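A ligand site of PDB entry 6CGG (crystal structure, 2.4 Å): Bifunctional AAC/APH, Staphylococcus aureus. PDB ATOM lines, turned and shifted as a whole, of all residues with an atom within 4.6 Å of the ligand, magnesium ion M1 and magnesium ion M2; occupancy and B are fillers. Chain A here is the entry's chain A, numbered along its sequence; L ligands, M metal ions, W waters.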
ATOM      1  N   ILE A  34      37.936  24.580  10.582  1.00  0.00           N
ATOM      2  CA  ILE A  34      37.554  23.258  11.096  1.00  0.00           C
ATOM      3  C   ILE A  34      36.757  22.461  10.094  1.00  0.00           C
ATOM      4  O   ILE A  34      36.697  21.242  10.183  1.00  0.00           O
ATOM      5  CB  ILE A  34      36.894  23.358  12.489  1.00  0.00           C
ATOM      6  CG1 ILE A  34      36.895  21.977  13.130  1.00  0.00           C
ATOM      7  CG2 ILE A  34      35.519  24.026  12.427  1.00  0.00           C
ATOM      8  CD1 ILE A  34      36.810  21.973  14.640  1.00  0.00           C
ATOM      9  N   GLY A  35      36.130  23.139   9.145  1.00  0.00           N
ATOM     10  CA  GLY A  35      35.613  22.494   7.969  1.00  0.00           C
ATOM     11  C   GLY A  35      35.144  23.463   6.896  1.00  0.00           C
ATOM     12  O   GLY A  35      35.039  24.683   7.106  1.00  0.00           O
ATOM     13  N   SER A  36      34.808  22.889   5.754  1.00  0.00           N
ATOM     14  CA  SER A  36      34.267  23.692   4.675  1.00  0.00           C
ATOM     15  C   SER A  36      33.380  22.896   3.683  1.00  0.00           C
ATOM     16  O   SER A  36      33.575  21.692   3.465  1.00  0.00           O
ATOM     17  CB  SER A  36      35.420  24.335   3.879  1.00  0.00           C
ATOM     18  OG  SER A  36      36.018  23.352   3.039  1.00  0.00           O
ATOM     19  N   GLY A  37      32.437  23.607   3.083  1.00  0.00           N
ATOM     20  CA  GLY A  37      31.648  23.100   1.998  1.00  0.00           C
ATOM     21  C   GLY A  37      32.225  23.713   0.773  1.00  0.00           C
ATOM     22  O   GLY A  37      33.439  24.001   0.691  1.00  0.00           O
ATOM     23  N   SER A  40      30.908  27.648   1.665  1.00  0.00           N
ATOM     24  CA  SER A  40      30.985  28.072   3.042  1.00  0.00           C
ATOM     25  C   SER A  40      32.283  27.636   3.690  1.00  0.00           C
ATOM     26  O   SER A  40      32.904  26.681   3.242  1.00  0.00           O
ATOM     27  CB  SER A  40      29.785  27.436   3.822  1.00  0.00           C
ATOM     28  OG  SER A  40      29.945  26.041   3.963  1.00  0.00           O
ATOM     29  N   ALA A  42      33.852  27.029   7.826  1.00  0.00           N
ATOM     30  CA  ALA A  42      33.702  27.015   9.279  1.00  0.00           C
ATOM     31  C   ALA A  42      35.053  27.043  10.068  1.00  0.00           C
ATOM     32  O   ALA A  42      36.007  26.370   9.728  1.00  0.00           O
ATOM     33  CB  ALA A  42      32.902  25.784   9.687  1.00  0.00           C
ATOM     34  N   ILE A  50      32.248  27.814  17.448  1.00  0.00           N
ATOM     35  CA  ILE A  50      32.240  27.522  16.035  1.00  0.00           C
ATOM     36  C   ILE A  50      31.688  28.781  15.404  1.00  0.00           C
ATOM     37  O   ILE A  50      30.720  29.350  15.940  1.00  0.00           O
ATOM     38  CB  ILE A  50      31.266  26.408  15.679  1.00  0.00           C
ATOM     39  CG1 ILE A  50      31.699  25.073  16.316  1.00  0.00           C
ATOM     40  CG2 ILE A  50      31.174  26.230  14.167  1.00  0.00           C
ATOM     41  CD1 ILE A  50      32.878  24.403  15.667  1.00  0.00           C
ATOM     42  N   LYS A  52      30.355  29.603  11.600  1.00  0.00           N
ATOM     43  CA  LYS A  52      30.021  29.192  10.231  1.00  0.00           C
ATOM     44  C   LYS A  52      29.905  30.476   9.414  1.00  0.00           C
ATOM     45  O   LYS A  52      29.298  31.450   9.890  1.00  0.00           O
ATOM     46  CB  LYS A  52      28.669  28.537  10.159  1.00  0.00           C
ATOM     47  CG  LYS A  52      28.600  27.179  10.817  1.00  0.00           C
ATOM     48  CD  LYS A  52      27.254  26.474  10.668  1.00  0.00           C
ATOM     49  CE  LYS A  52      27.006  26.085   9.219  1.00  0.00           C
ATOM     50  NZ  LYS A  52      25.935  25.000   9.155  1.00  0.00           N
ATOM     51  N   TYR A  63      22.057  32.032   5.765  1.00  0.00           N
ATOM     52  CA  TYR A  63      21.970  31.591   7.192  1.00  0.00           C
ATOM     53  C   TYR A  63      20.817  32.100   8.076  1.00  0.00           C
ATOM     54  O   TYR A  63      20.695  31.696   9.213  1.00  0.00           O
ATOM     55  CB  TYR A  63      23.293  31.796   7.898  1.00  0.00           C
ATOM     56  CG  TYR A  63      24.445  30.883   7.463  1.00  0.00           C
ATOM     57  CD1 TYR A  63      24.227  29.699   6.696  1.00  0.00           C
ATOM     58  CD2 TYR A  63      25.749  31.167   7.875  1.00  0.00           C
ATOM     59  CE1 TYR A  63      25.273  28.921   6.304  1.00  0.00           C
ATOM     60  CE2 TYR A  63      26.823  30.342   7.491  1.00  0.00           C
ATOM     61  CZ  TYR A  63      26.583  29.232   6.727  1.00  0.00           C
ATOM     62  OH  TYR A  63      27.593  28.407   6.361  1.00  0.00           O
ATOM     63  N   GLU A  66      18.607  28.909   8.829  1.00  0.00           N
ATOM     64  CA  GLU A  66      19.311  28.056   9.758  1.00  0.00           C
ATOM     65  C   GLU A  66      19.235  28.611  11.191  1.00  0.00           C
ATOM     66  O   GLU A  66      19.038  27.858  12.160  1.00  0.00           O
ATOM     67  CB  GLU A  66      20.761  27.870   9.317  1.00  0.00           C
ATOM     68  CG  GLU A  66      21.568  26.970  10.238  1.00  0.00           C
ATOM     69  CD  GLU A  66      22.849  26.420   9.624  1.00  0.00           C
ATOM     70  OE1 GLU A  66      23.097  26.634   8.361  1.00  0.00           O
ATOM     71  OE2 GLU A  66      23.536  25.717  10.395  1.00  0.00           O
ATOM     72  N   TYR A 100      28.344  29.977  17.710  1.00  0.00           N
ATOM     73  CA  TYR A 100      27.779  29.253  18.832  1.00  0.00           C
ATOM     74  C   TYR A 100      28.885  28.453  19.506  1.00  0.00           C
ATOM     75  O   TYR A 100      29.937  28.208  18.879  1.00  0.00           O
ATOM     76  CB  TYR A 100      26.651  28.297  18.314  1.00  0.00           C
ATOM     77  CG  TYR A 100      27.078  27.320  17.234  1.00  0.00           C
ATOM     78  CD1 TYR A 100      27.572  26.088  17.551  1.00  0.00           C
ATOM     79  CD2 TYR A 100      26.942  27.606  15.905  1.00  0.00           C
ATOM     80  CE1 TYR A 100      27.919  25.165  16.583  1.00  0.00           C
ATOM     81  CE2 TYR A 100      27.301  26.691  14.891  1.00  0.00           C
ATOM     82  CZ  TYR A 100      27.780  25.484  15.238  1.00  0.00           C
ATOM     83  OH  TYR A 100      28.140  24.558  14.252  1.00  0.00           O
ATOM     84  N   LYS A 101      28.654  28.026  20.752  1.00  0.00           N
ATOM     85  CA  LYS A 101      29.657  27.193  21.428  1.00  0.00           C
ATOM     86  C   LYS A 101      29.782  25.817  20.830  1.00  0.00           C
ATOM     87  O   LYS A 101      28.790  25.175  20.524  1.00  0.00           O
ATOM     88  CB  LYS A 101      29.370  27.065  22.901  1.00  0.00           C
ATOM     89  CG  LYS A 101      29.464  28.367  23.671  1.00  0.00           C
ATOM     90  CD  LYS A 101      29.985  28.101  25.065  1.00  0.00           C
ATOM     91  CE  LYS A 101      30.292  29.345  25.883  1.00  0.00           C
ATOM     92  NZ  LYS A 101      29.000  29.997  26.205  1.00  0.00           N
ATOM     93  N   GLU A 102      31.019  25.391  20.612  1.00  0.00           N
ATOM     94  CA  GLU A 102      31.367  24.110  20.026  1.00  0.00           C
ATOM     95  C   GLU A 102      30.744  23.056  20.941  1.00  0.00           C
ATOM     96  O   GLU A 102      30.918  23.077  22.129  1.00  0.00           O
ATOM     97  CB  GLU A 102      32.890  23.902  20.037  1.00  0.00           C
ATOM     98  CG  GLU A 102      33.369  22.590  19.454  1.00  0.00           C
ATOM     99  CD  GLU A 102      34.819  22.267  19.742  1.00  0.00           C
ATOM    100  OE1 GLU A 102      35.302  22.710  20.792  1.00  0.00           O
ATOM    101  OE2 GLU A 102      35.510  21.574  18.945  1.00  0.00           O
ATOM    102  N   ILE A 103      30.029  22.110  20.352  1.00  0.00           N
ATOM    103  CA  ILE A 103      29.603  20.929  21.094  1.00  0.00           C
ATOM    104  C   ILE A 103      30.742  19.969  21.101  1.00  0.00           C
ATOM    105  O   ILE A 103      31.268  19.665  20.048  1.00  0.00           O
ATOM    106  CB  ILE A 103      28.361  20.304  20.431  1.00  0.00           C
ATOM    107  CG1 ILE A 103      27.192  21.283  20.510  1.00  0.00           C
ATOM    108  CG2 ILE A 103      27.973  19.008  21.136  1.00  0.00           C
ATOM    109  CD1 ILE A 103      26.112  20.938  19.511  1.00  0.00           C
ATOM    110  N   PHE A 107      32.959  12.591  16.309  1.00  0.00           N
ATOM    111  CA  PHE A 107      32.016  12.341  15.265  1.00  0.00           C
ATOM    112  C   PHE A 107      31.945  10.876  14.968  1.00  0.00           C
ATOM    113  O   PHE A 107      32.937  10.205  14.900  1.00  0.00           O
ATOM    114  CB  PHE A 107      32.307  13.162  13.990  1.00  0.00           C
ATOM    115  CG  PHE A 107      31.872  14.587  14.096  1.00  0.00           C
ATOM    116  CD1 PHE A 107      30.528  14.900  14.021  1.00  0.00           C
ATOM    117  CD2 PHE A 107      32.816  15.578  14.367  1.00  0.00           C
ATOM    118  CE1 PHE A 107      30.121  16.222  14.185  1.00  0.00           C
ATOM    119  CE2 PHE A 107      32.430  16.905  14.511  1.00  0.00           C
ATOM    120  CZ  PHE A 107      31.086  17.248  14.433  1.00  0.00           C
ATOM    121  N   ASP A 200      19.737  16.476   6.651  1.00  0.00           N
ATOM    122  CA  ASP A 200      21.093  16.101   6.200  1.00  0.00           C
ATOM    123  C   ASP A 200      21.724  15.251   7.268  1.00  0.00           C
ATOM    124  O   ASP A 200      22.808  15.528   7.741  1.00  0.00           O
ATOM    125  CB  ASP A 200      21.874  17.369   5.951  1.00  0.00           C
ATOM    126  CG  ASP A 200      23.145  17.171   5.128  1.00  0.00           C
ATOM    127  OD1 ASP A 200      23.500  16.035   4.690  1.00  0.00           O
ATOM    128  OD2 ASP A 200      23.802  18.257   4.960  1.00  0.00           O
ATOM    129  N   ASN A 204      28.543  12.089   9.828  1.00  0.00           N
ATOM    130  CA  ASN A 204      29.462  13.245  10.057  1.00  0.00           C
ATOM    131  C   ASN A 204      28.784  14.471  10.758  1.00  0.00           C
ATOM    132  O   ASN A 204      29.414  15.480  11.032  1.00  0.00           O
ATOM    133  CB  ASN A 204      30.217  13.631   8.760  1.00  0.00           C
ATOM    134  CG  ASN A 204      29.343  14.427   7.782  1.00  0.00           C
ATOM    135  OD1 ASN A 204      28.154  14.277   7.745  1.00  0.00           O
ATOM    136  ND2 ASN A 204      29.928  15.191   7.010  1.00  0.00           N
ATOM    137  N   HIS A 205      27.511  14.392  11.076  1.00  0.00           N
ATOM    138  CA  HIS A 205      26.845  15.415  11.867  1.00  0.00           C
ATOM    139  C   HIS A 205      26.429  14.919  13.237  1.00  0.00           C
ATOM    140  O   HIS A 205      25.755  15.635  13.936  1.00  0.00           O
ATOM    141  CB  HIS A 205      25.641  15.945  11.141  1.00  0.00           C
ATOM    142  CG  HIS A 205      25.948  16.711   9.920  1.00  0.00           C
ATOM    143  ND1 HIS A 205      25.101  16.780   8.847  1.00  0.00           N
ATOM    144  CD2 HIS A 205      27.016  17.493   9.594  1.00  0.00           C
ATOM    145  CE1 HIS A 205      25.623  17.555   7.894  1.00  0.00           C
ATOM    146  NE2 HIS A 205      26.783  17.987   8.334  1.00  0.00           N
ATOM    147  N   LEU A 207      27.501  13.540  17.018  1.00  0.00           N
ATOM    148  CA  LEU A 207      28.582  13.546  17.977  1.00  0.00           C
ATOM    149  C   LEU A 207      28.342  12.541  19.103  1.00  0.00           C
ATOM    150  O   LEU A 207      27.221  12.471  19.707  1.00  0.00           O
ATOM    151  CB  LEU A 207      28.702  14.929  18.588  1.00  0.00           C
ATOM    152  CG  LEU A 207      29.424  15.967  17.717  1.00  0.00           C
ATOM    153  CD1 LEU A 207      29.149  17.376  18.192  1.00  0.00           C
ATOM    154  CD2 LEU A 207      30.940  15.776  17.696  1.00  0.00           C
ATOM    155  N   ILE A 218      24.679  18.506  14.805  1.00  0.00           N
ATOM    156  CA  ILE A 218      24.967  19.798  14.202  1.00  0.00           C
ATOM    157  C   ILE A 218      24.427  19.867  12.819  1.00  0.00           C
ATOM    158  O   ILE A 218      23.929  18.870  12.265  1.00  0.00           O
ATOM    159  CB  ILE A 218      26.499  20.031  14.103  1.00  0.00           C
ATOM    160  CG1 ILE A 218      27.167  18.882  13.328  1.00  0.00           C
ATOM    161  CG2 ILE A 218      27.134  20.164  15.491  1.00  0.00           C
ATOM    162  CD1 ILE A 218      28.548  19.257  12.916  1.00  0.00           C
ATOM    163  N   ASP A 219      24.521  21.056  12.262  1.00  0.00           N
ATOM    164  CA  ASP A 219      24.222  21.367  10.857  1.00  0.00           C
ATOM    165  C   ASP A 219      22.764  21.074  10.502  1.00  0.00           C
ATOM    166  O   ASP A 219      22.471  20.124   9.748  1.00  0.00           O
ATOM    167  CB  ASP A 219      25.190  20.707   9.897  1.00  0.00           C
ATOM    168  CG  ASP A 219      25.107  21.274   8.480  1.00  0.00           C
ATOM    169  OD1 ASP A 219      24.151  22.020   8.156  1.00  0.00           O
ATOM    170  OD2 ASP A 219      26.022  20.963   7.621  1.00  0.00           O
HETATM  171  P1  LIG L   1      26.741  24.515   5.213  1.00  0.00           P
HETATM  172  O1  LIG L   1      26.411  26.103   5.003  1.00  0.00           O
HETATM  173  O2  LIG L   1      26.676  23.767   3.951  1.00  0.00           O
HETATM  174  O3  LIG L   1      25.672  24.004   6.422  1.00  0.00           O
HETATM  175  N1  LIG L   1      28.142  24.363   6.034  1.00  0.00           N
HETATM  176  P2  LIG L   1      28.811  22.988   6.546  1.00  0.00           P
HETATM  177  O4  LIG L   1      30.316  22.648   6.229  1.00  0.00           O
HETATM  178  O5  LIG L   1      28.298  21.900   5.736  1.00  0.00           O
HETATM  179  O6  LIG L   1      28.789  23.166   8.075  1.00  0.00           O
HETATM  180  P3  LIG L   1      28.664  22.275   9.381  1.00  0.00           P
HETATM  181  O7  LIG L   1      27.613  22.939  10.238  1.00  0.00           O
HETATM  182  O8  LIG L   1      28.530  20.833   9.046  1.00  0.00           O
HETATM  183  O9  LIG L   1      30.101  22.503  10.185  1.00  0.00           O
HETATM  184  C1  LIG L   1      31.256  22.206   9.439  1.00  0.00           C
HETATM  185  C2  LIG L   1      32.149  21.369  10.316  1.00  0.00           C
HETATM  186  O10 LIG L   1      32.454  22.128  11.496  1.00  0.00           O
HETATM  187  C3  LIG L   1      31.569  20.080  10.831  1.00  0.00           C
HETATM  188  O11 LIG L   1      31.837  19.008   9.996  1.00  0.00           O
HETATM  189  C4  LIG L   1      32.397  19.845  12.083  1.00  0.00           C
HETATM  190  O12 LIG L   1      33.727  19.368  11.846  1.00  0.00           O
HETATM  191  C5  LIG L   1      32.529  21.264  12.623  1.00  0.00           C
HETATM  192  N2  LIG L   1      31.479  21.663  13.587  1.00  0.00           N
HETATM  193  C6  LIG L   1      30.464  22.584  13.494  1.00  0.00           C
HETATM  194  N3  LIG L   1      29.835  22.806  14.629  1.00  0.00           N
HETATM  195  C7  LIG L   1      30.469  21.951  15.517  1.00  0.00           C
HETATM  196  C8  LIG L   1      30.260  21.709  16.884  1.00  0.00           C
HETATM  197  O13 LIG L   1      29.344  22.118  17.580  1.00  0.00           O
HETATM  198  N4  LIG L   1      31.196  20.832  17.393  1.00  0.00           N
HETATM  199  C9  LIG L   1      32.207  20.239  16.662  1.00  0.00           C
HETATM  200  N5  LIG L   1      32.974  19.334  17.289  1.00  0.00           N
HETATM  201  N6  LIG L   1      32.384  20.438  15.365  1.00  0.00           N
HETATM  202  C10 LIG L   1      31.502  21.269  14.870  1.00  0.00           C
HETATM  203 MG    MG M   1      27.846  19.990   7.410  1.00  0.00          MG
HETATM  204 MG    MG M   2      25.324  22.191   6.282  1.00  0.00          MG
HETATM  205  O   HOH W   1      31.380  20.435   6.041  1.00  0.00           O
HETATM  206  O   HOH W   2      23.038  26.325   5.733  1.00  0.00           O
HETATM  207  O   HOH W   3      24.890  24.620   1.136  1.00  0.00           O
HETATM  208  O   HOH W   4      35.545  19.197  15.171  1.00  0.00           O
HETATM  209  O   HOH W   5      25.405  21.387   4.458  1.00  0.00           O
HETATM  210  O   HOH W   6      31.457  25.340   5.891  1.00  0.00           O
HETATM  211  O   HOH W   7      34.793  18.745  19.869  1.00  0.00           O
HETATM  212  O   HOH W   8      31.908  16.119  10.695  1.00  0.00           O
HETATM  213  O   HOH W   9      29.395  18.787   7.321  1.00  0.00           O
HETATM  214  O   HOH W  10      28.995  20.964   3.448  1.00  0.00           O
HETATM  215  O   HOH W  11      27.530  19.739   5.659  1.00  0.00           O
HETATM  216  O   HOH W  12      23.277  20.567   5.970  1.00  0.00           O
HETATM  217  O   HOH W  13      26.526  23.184  12.638  1.00  0.00           O
HETATM  218  O   HOH W  14      35.138  16.880  17.249  1.00  0.00           O
HETATM  219  O   HOH W  15      23.247  23.221   5.556  1.00  0.00           O
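One residue has an atom within 4 Å of magnesium ion M2: Asp 219.
Ile 34 touches the ligand. C of Ser 36 touches O4 of the ligand, at 3.99 Å. Gly 37 touches the ligand. Ala 42 touches the ligand (CB to C1, 3.9 Å). Ile 50 touches the ligand (CG1 to N3, 3.4 Å). CG of Glu 102 touches N4 of the ligand, at 3.5 Å. CZ of Phe 107 touches N6 of the ligand, 3.6 Å away. Ile 218 touches the ligand (CG2 to O13, 3.6 Å). Hydrophobic or aromatic side chains that line the ligand: Ile 34, Ala 42, Ile 50, Tyr 63, Tyr 100, Ile 103, Phe 107, His 205 and Ile 218. The nearest printed residue that does not touch the ligand is Leu 207 (4.1 Å).
OG of Ser 40 lies within hydrogen-bond range of N1 of the ligand (3.2 Å). An oxygen (O7) of the ligand is in salt-bridge range of the side-chain amino group (NZ) of Lys 52 (2.9 Å). The side-chain hydroxyl (OH) of Tyr 100 lies within hydrogen-bond range of a nitrogen (N3) of the ligand (2.5 Å). The backbone carbonyl oxygen (O) of Ile 103 lies within hydrogen-bond range of a nitrogen (N4) of the ligand, at 2.9 Å. An oxygen (O13) of the ligand lies within hydrogen-bond range of the backbone NH (N) of Ile 103, 2.9 Å away. An oxygen (O1) of the ligand is in hydrogen-bond range of the side-chain hydroxyl (OH) of Tyr 63 (2.9 Å).
Water W13 lies within hydrogen-bond range of an oxygen (O7) of the ligand (2.6 Å), the side-chain hydroxyl of Tyr 100 (2.7 Å) and the backbone NH of Asp 219 (2.9 Å). Water W6 lies within hydrogen-bond range of OG of Ser 40 (2.5 Å), O4 of the ligand (2.9 Å) and N of Gly 37 (3.4 Å). Water W8 bridges O of Asn 204 and O11 of the ligand. Water W7 lies within hydrogen-bond range of the side-chain carboxylate of Glu 102 and a nitrogen (N5) of the ligand. Water W2 bridges the side-chain carboxylate (OE1) of Glu 66 and an oxygen (O1) of the ligand.
Within 4 Å of magnesium ion M1: His 205 and Asp 219. The nearest printed residue that does not touch magnesium ion M1 is Asp 200 (5.0 Å).
Magnesium ion M1 is bound by water W11 (1.8 Å), an oxygen (O8) of the ligand (2.0 Å), water W9 (2.0 Å), the side-chain carboxylate (OD2) of Asp 219 (2.1 Å), a ring nitrogen (NE2) of His 205 (2.4 Å) and an oxygen (O5) of the ligand (2.6 Å). Magnesium ion M1 has six donor atoms within binding distance.
The side-chain amino group (NZ) of Lys 52 lies within salt-bridge range of the side-chain carboxylate (OE2) of Glu 66 (2.8 Å). ND1 of His 205 is in hydrogen-bond range of O of Asp 200, 2.8 Å away. N of Ala 42 sits at hydrogen-bond distance from O of Gly 35, at 2.7 Å. The backbone NH (N) of Ile 50 is in hydrogen-bond range of the backbone carbonyl oxygen (O) of Tyr 100 (2.7 Å). The backbone NH (N) of Ile 218 lies within hydrogen-bond range of the backbone carbonyl oxygen (O) of His 205. N of Ile 34 lies within hydrogen-bond range of O of Ala 42, at 2.8 Å. OD1 of Asp 219 lies close to NZ of Lys 52 (3.6 Å).
Magnesium ion M2 is bound by an oxygen (O3) of the ligand (1.9 Å), the side-chain carboxylate (OD2) of Asp 219 (1.9 Å), water W5 (2.0 Å), the side-chain carboxylate (OD1) of Asp 219 (2.2 Å) and water W15 (2.4 Å). Magnesium ion M2 has five donor atoms within binding distance. Slightly farther from magnesium ion M2 lies water W12 (2.6 Å).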
